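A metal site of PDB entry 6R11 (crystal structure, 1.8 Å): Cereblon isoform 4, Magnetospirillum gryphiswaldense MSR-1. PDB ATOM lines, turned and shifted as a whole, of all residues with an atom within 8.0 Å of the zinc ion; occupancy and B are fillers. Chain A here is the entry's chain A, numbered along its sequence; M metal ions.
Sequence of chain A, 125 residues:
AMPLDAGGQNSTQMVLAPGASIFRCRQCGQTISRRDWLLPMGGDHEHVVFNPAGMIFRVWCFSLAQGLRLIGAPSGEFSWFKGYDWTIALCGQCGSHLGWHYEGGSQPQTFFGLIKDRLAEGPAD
The side-chain sulfur (SG) of Cys 25 sits close to the backbone NH (N) of Gln 27 (3.5 Å). The backbone carbonyl oxygen of Gln 30 sits at hydrogen-bond distance from the backbone NH of Cys 25 (2.8 Å). N of Ser 96 sits close to SG of Cys 94 (3.5 Å). SG of Cys 28 lies close to N of Gln 30. The side-chain sulfur (SG) of Cys 28 sits close to the side-chain amide nitrogen (NE2) of Gln 93, at 3.2 Å. The backbone NH (N) of Cys 91 lies within hydrogen-bond range of the backbone carbonyl oxygen (O) of Ser 96, 2.7 Å away. The backbone NH (N) of Gln 93 lies close to the side-chain sulfur (SG) of Cys 91 (3.5 Å).
The zinc ion is bound by SG of Cys 25 (2.3 Å), SG of Cys 94 (2.3 Å), SG of Cys 28 (2.3 Å) and SG of Cys 91 (2.3 Å).
Of the 21 residues printed, 4 come within 4 Å of the zinc ion.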
ATOM      1  N   ARG A  24     -30.043 -22.551  26.790  1.00  0.00           N
ATOM      2  CA  ARG A  24     -28.637 -22.519  27.090  1.00  0.00           C
ATOM      3  C   ARG A  24     -27.841 -22.341  25.814  1.00  0.00           C
ATOM      4  O   ARG A  24     -28.304 -22.664  24.756  1.00  0.00           O
ATOM      5  CB  ARG A  24     -28.236 -23.850  27.732  1.00  0.00           C
ATOM      6  CG  ARG A  24     -28.891 -24.082  29.078  1.00  0.00           C
ATOM      7  CD  ARG A  24     -28.375 -25.359  29.771  1.00  0.00           C
ATOM      8  NE  ARG A  24     -28.933 -25.387  31.120  1.00  0.00           N
ATOM      9  CZ  ARG A  24     -28.518 -24.664  32.167  1.00  0.00           C
ATOM     10  NH1 ARG A  24     -27.424 -23.918  32.107  1.00  0.00           N
ATOM     11  NH2 ARG A  24     -29.188 -24.725  33.291  1.00  0.00           N
ATOM     12  N   CYS A  25     -26.601 -21.825  25.923  1.00  0.00           N
ATOM     13  CA  CYS A  25     -25.693 -21.843  24.826  1.00  0.00           C
ATOM     14  C   CYS A  25     -25.478 -23.283  24.292  1.00  0.00           C
ATOM     15  O   CYS A  25     -25.148 -24.184  25.061  1.00  0.00           O
ATOM     16  CB  CYS A  25     -24.386 -21.211  25.241  1.00  0.00           C
ATOM     17  SG  CYS A  25     -23.088 -21.266  23.906  1.00  0.00           S
ATOM     18  N   ARG A  26     -25.694 -23.459  22.978  1.00  0.00           N
ATOM     19  CA  ARG A  26     -25.533 -24.762  22.363  1.00  0.00           C
ATOM     20  C   ARG A  26     -24.109 -25.326  22.444  1.00  0.00           C
ATOM     21  O   ARG A  26     -23.917 -26.543  22.438  1.00  0.00           O
ATOM     22  CB  ARG A  26     -25.988 -24.675  20.895  1.00  0.00           C
ATOM     23  CG  ARG A  26     -25.766 -25.915  20.093  1.00  0.00           C
ATOM     24  CD  ARG A  26     -26.315 -25.694  18.722  1.00  0.00           C
ATOM     25  NE  ARG A  26     -25.942 -26.846  17.935  1.00  0.00           N
ATOM     26  CZ  ARG A  26     -26.259 -27.002  16.652  1.00  0.00           C
ATOM     27  NH1 ARG A  26     -26.988 -26.064  16.033  1.00  0.00           N
ATOM     28  NH2 ARG A  26     -25.819 -28.074  16.018  1.00  0.00           N
ATOM     29  N   GLN A  27     -23.120 -24.446  22.500  1.00  0.00           N
ATOM     30  CA  GLN A  27     -21.712 -24.861  22.532  1.00  0.00           C
ATOM     31  C   GLN A  27     -21.168 -25.237  23.889  1.00  0.00           C
ATOM     32  O   GLN A  27     -20.315 -26.088  23.971  1.00  0.00           O
ATOM     33  CB  GLN A  27     -20.834 -23.784  21.887  1.00  0.00           C
ATOM     34  CG  GLN A  27     -21.278 -23.448  20.485  1.00  0.00           C
ATOM     35  CD  GLN A  27     -21.247 -24.653  19.540  1.00  0.00           C
ATOM     36  OE1 GLN A  27     -20.388 -25.541  19.662  1.00  0.00           O
ATOM     37  NE2 GLN A  27     -22.241 -24.738  18.651  1.00  0.00           N
ATOM     38  N   CYS A  28     -21.654 -24.600  24.964  1.00  0.00           N
ATOM     39  CA  CYS A  28     -21.044 -24.770  26.275  1.00  0.00           C
ATOM     40  C   CYS A  28     -22.033 -24.943  27.439  1.00  0.00           C
ATOM     41  O   CYS A  28     -21.636 -25.287  28.575  1.00  0.00           O
ATOM     42  CB  CYS A  28     -20.063 -23.636  26.531  1.00  0.00           C
ATOM     43  SG  CYS A  28     -20.972 -22.137  26.975  1.00  0.00           S
ATOM     44  N   GLY A  29     -23.324 -24.722  27.201  1.00  0.00           N
ATOM     45  CA  GLY A  29     -24.330 -24.884  28.187  1.00  0.00           C
ATOM     46  C   GLY A  29     -24.583 -23.735  29.132  1.00  0.00           C
ATOM     47  O   GLY A  29     -25.423 -23.832  30.050  1.00  0.00           O
ATOM     48  N   GLN A  30     -23.914 -22.598  28.933  1.00  0.00           N
ATOM     49  CA  GLN A  30     -24.205 -21.388  29.723  1.00  0.00           C
ATOM     50  C   GLN A  30     -25.699 -21.087  29.708  1.00  0.00           C
ATOM     51  O   GLN A  30     -26.289 -21.093  28.653  1.00  0.00           O
ATOM     52  CB  GLN A  30     -23.467 -20.182  29.110  1.00  0.00           C
ATOM     53  CG  GLN A  30     -23.759 -18.826  29.742  1.00  0.00           C
ATOM     54  CD  GLN A  30     -22.793 -18.477  30.823  1.00  0.00           C
ATOM     55  OE1 GLN A  30     -22.534 -19.268  31.694  1.00  0.00           O
ATOM     56  NE2 GLN A  30     -22.255 -17.272  30.780  1.00  0.00           N
ATOM     57  N   THR A  31     -26.275 -20.772  30.859  1.00  0.00           N
ATOM     58  CA  THR A  31     -27.711 -20.361  30.919  1.00  0.00           C
ATOM     59  C   THR A  31     -27.856 -19.016  30.246  1.00  0.00           C
ATOM     60  O   THR A  31     -27.089 -18.119  30.553  1.00  0.00           O
ATOM     61  CB  THR A  31     -28.198 -20.202  32.385  1.00  0.00           C
ATOM     62  OG1 THR A  31     -27.717 -21.268  33.233  1.00  0.00           O
ATOM     63  CG2 THR A  31     -29.668 -20.157  32.410  1.00  0.00           C
ATOM     64  N   ILE A  32     -28.792 -18.886  29.327  1.00  0.00           N
ATOM     65  CA  ILE A  32     -28.945 -17.653  28.571  1.00  0.00           C
ATOM     66  C   ILE A  32     -30.331 -17.033  28.761  1.00  0.00           C
ATOM     67  O   ILE A  32     -30.439 -15.836  28.994  1.00  0.00           O
ATOM     68  CB  ILE A  32     -28.701 -17.847  27.053  1.00  0.00           C
ATOM     69  CG1 ILE A  32     -27.295 -18.373  26.764  1.00  0.00           C
ATOM     70  CG2 ILE A  32     -28.876 -16.510  26.313  1.00  0.00           C
ATOM     71  CD1 ILE A  32     -26.121 -17.498  27.236  1.00  0.00           C
ATOM     72  N   GLY A  67     -25.964 -14.214  31.054  1.00  0.00           N
ATOM     73  CA  GLY A  67     -24.829 -15.038  30.682  1.00  0.00           C
ATOM     74  C   GLY A  67     -24.138 -14.623  29.393  1.00  0.00           C
ATOM     75  O   GLY A  67     -23.328 -15.387  28.844  1.00  0.00           O
ATOM     76  N   LEU A  68     -24.470 -13.464  28.876  1.00  0.00           N
ATOM     77  CA  LEU A  68     -23.881 -12.937  27.639  1.00  0.00           C
ATOM     78  C   LEU A  68     -22.829 -11.916  27.983  1.00  0.00           C
ATOM     79  O   LEU A  68     -22.706 -11.513  29.138  1.00  0.00           O
ATOM     80  CB  LEU A  68     -24.964 -12.240  26.783  1.00  0.00           C
ATOM     81  CG  LEU A  68     -26.080 -13.143  26.298  1.00  0.00           C
ATOM     82  CD1 LEU A  68     -27.304 -12.364  25.904  1.00  0.00           C
ATOM     83  CD2 LEU A  68     -25.640 -14.146  25.207  1.00  0.00           C
ATOM     84  N   LEU A  90     -22.239 -11.977  22.708  1.00  0.00           N
ATOM     85  CA  LEU A  90     -21.561 -13.283  22.760  1.00  0.00           C
ATOM     86  C   LEU A  90     -21.947 -14.046  24.019  1.00  0.00           C
ATOM     87  O   LEU A  90     -22.284 -13.447  25.065  1.00  0.00           O
ATOM     88  CB  LEU A  90     -20.070 -13.059  22.755  1.00  0.00           C
ATOM     89  CG  LEU A  90     -19.512 -12.182  21.656  1.00  0.00           C
ATOM     90  CD1 LEU A  90     -17.986 -12.109  21.874  1.00  0.00           C
ATOM     91  CD2 LEU A  90     -19.964 -12.701  20.271  1.00  0.00           C
ATOM     92  N   CYS A  91     -21.877 -15.349  23.922  1.00  0.00           N
ATOM     93  CA  CYS A  91     -21.898 -16.167  25.140  1.00  0.00           C
ATOM     94  C   CYS A  91     -20.781 -15.715  26.026  1.00  0.00           C
ATOM     95  O   CYS A  91     -19.627 -15.644  25.607  1.00  0.00           O
ATOM     96  CB  CYS A  91     -21.682 -17.622  24.816  1.00  0.00           C
ATOM     97  SG  CYS A  91     -21.649 -18.720  26.255  1.00  0.00           S
ATOM     98  N   GLY A  92     -21.107 -15.373  27.280  1.00  0.00           N
ATOM     99  CA  GLY A  92     -20.076 -14.885  28.210  1.00  0.00           C
ATOM    100  C   GLY A  92     -19.085 -15.922  28.629  1.00  0.00           C
ATOM    101  O   GLY A  92     -18.011 -15.580  29.141  1.00  0.00           O
ATOM    102  N   GLN A  93     -19.427 -17.190  28.435  1.00  0.00           N
ATOM    103  CA  GLN A  93     -18.584 -18.289  28.825  1.00  0.00           C
ATOM    104  C   GLN A  93     -17.606 -18.658  27.710  1.00  0.00           C
ATOM    105  O   GLN A  93     -16.399 -18.683  27.906  1.00  0.00           O
ATOM    106  CB  GLN A  93     -19.454 -19.458  29.251  1.00  0.00           C
ATOM    107  CG  GLN A  93     -18.697 -20.634  29.795  1.00  0.00           C
ATOM    108  CD  GLN A  93     -19.556 -21.514  30.691  1.00  0.00           C
ATOM    109  OE1 GLN A  93     -19.479 -21.357  31.928  1.00  0.00           O
ATOM    110  NE2 GLN A  93     -20.409 -22.360  30.110  1.00  0.00           N
ATOM    111  N   CYS A  94     -18.158 -18.940  26.530  1.00  0.00           N
ATOM    112  CA  CYS A  94     -17.360 -19.509  25.437  1.00  0.00           C
ATOM    113  C   CYS A  94     -17.098 -18.594  24.259  1.00  0.00           C
ATOM    114  O   CYS A  94     -16.284 -18.954  23.395  1.00  0.00           O
ATOM    115  CB  CYS A  94     -17.955 -20.817  24.919  1.00  0.00           C
ATOM    116  SG  CYS A  94     -19.412 -20.670  23.792  1.00  0.00           S
ATOM    117  N   GLY A  95     -17.770 -17.425  24.229  1.00  0.00           N
ATOM    118  CA  GLY A  95     -17.602 -16.507  23.137  1.00  0.00           C
ATOM    119  C   GLY A  95     -18.393 -16.747  21.858  1.00  0.00           C
ATOM    120  O   GLY A  95     -18.287 -15.951  20.909  1.00  0.00           O
ATOM    121  N   SER A  96     -19.233 -17.776  21.800  1.00  0.00           N
ATOM    122  CA  SER A  96     -20.123 -18.051  20.667  1.00  0.00           C
ATOM    123  C   SER A  96     -21.017 -16.843  20.405  1.00  0.00           C
ATOM    124  O   SER A  96     -21.541 -16.225  21.346  1.00  0.00           O
ATOM    125  CB  SER A  96     -20.965 -19.305  20.896  1.00  0.00           C
ATOM    126  OG  SER A  96     -21.920 -19.525  19.848  1.00  0.00           O
ATOM    127  N   HIS A  97     -21.175 -16.467  19.120  1.00  0.00           N
ATOM    128  CA  HIS A  97     -22.047 -15.350  18.821  1.00  0.00           C
ATOM    129  C   HIS A  97     -23.490 -15.786  18.894  1.00  0.00           C
ATOM    130  O   HIS A  97     -23.947 -16.522  18.029  1.00  0.00           O
ATOM    131  CB  HIS A  97     -21.704 -14.753  17.450  1.00  0.00           C
ATOM    132  CG  HIS A  97     -22.654 -13.688  17.053  1.00  0.00           C
ATOM    133  ND1 HIS A  97     -22.920 -13.392  15.735  1.00  0.00           N
ATOM    134  CD2 HIS A  97     -23.400 -12.822  17.793  1.00  0.00           C
ATOM    135  CE1 HIS A  97     -23.789 -12.395  15.687  1.00  0.00           C
ATOM    136  NE2 HIS A  97     -24.102 -12.045  16.917  1.00  0.00           N
ATOM    137  N   LEU A  98     -24.212 -15.341  19.924  1.00  0.00           N
ATOM    138  CA  LEU A  98     -25.570 -15.786  20.178  1.00  0.00           C
ATOM    139  C   LEU A  98     -26.677 -14.900  19.632  1.00  0.00           C
ATOM    140  O   LEU A  98     -27.790 -15.370  19.429  1.00  0.00           O
ATOM    141  CB  LEU A  98     -25.778 -16.079  21.647  1.00  0.00           C
ATOM    142  CG  LEU A  98     -24.906 -17.220  22.202  1.00  0.00           C
ATOM    143  CD1 LEU A  98     -25.335 -17.570  23.606  1.00  0.00           C
ATOM    144  CD2 LEU A  98     -24.970 -18.484  21.380  1.00  0.00           C
ATOM    145  N   ARG A 118     -28.554 -21.460  17.690  1.00  0.00           N
ATOM    146  CA  ARG A 118     -27.358 -21.367  18.502  1.00  0.00           C
ATOM    147  C   ARG A 118     -27.635 -21.601  19.997  1.00  0.00           C
ATOM    148  O   ARG A 118     -26.716 -21.531  20.834  1.00  0.00           O
ATOM    149  CB  ARG A 118     -26.680 -20.028  18.277  1.00  0.00           C
ATOM    150  CG  ARG A 118     -26.210 -19.979  16.832  1.00  0.00           C
ATOM    151  CD  ARG A 118     -25.305 -18.835  16.497  1.00  0.00           C
ATOM    152  NE  ARG A 118     -25.122 -18.718  15.055  1.00  0.00           N
ATOM    153  CZ  ARG A 118     -24.302 -17.845  14.461  1.00  0.00           C
ATOM    154  NH1 ARG A 118     -23.574 -16.968  15.196  1.00  0.00           N
ATOM    155  NH2 ARG A 118     -24.188 -17.831  13.106  1.00  0.00           N
HETATM  156 ZN    ZN M   1     -21.261 -20.743  25.135  1.00  0.00          ZN
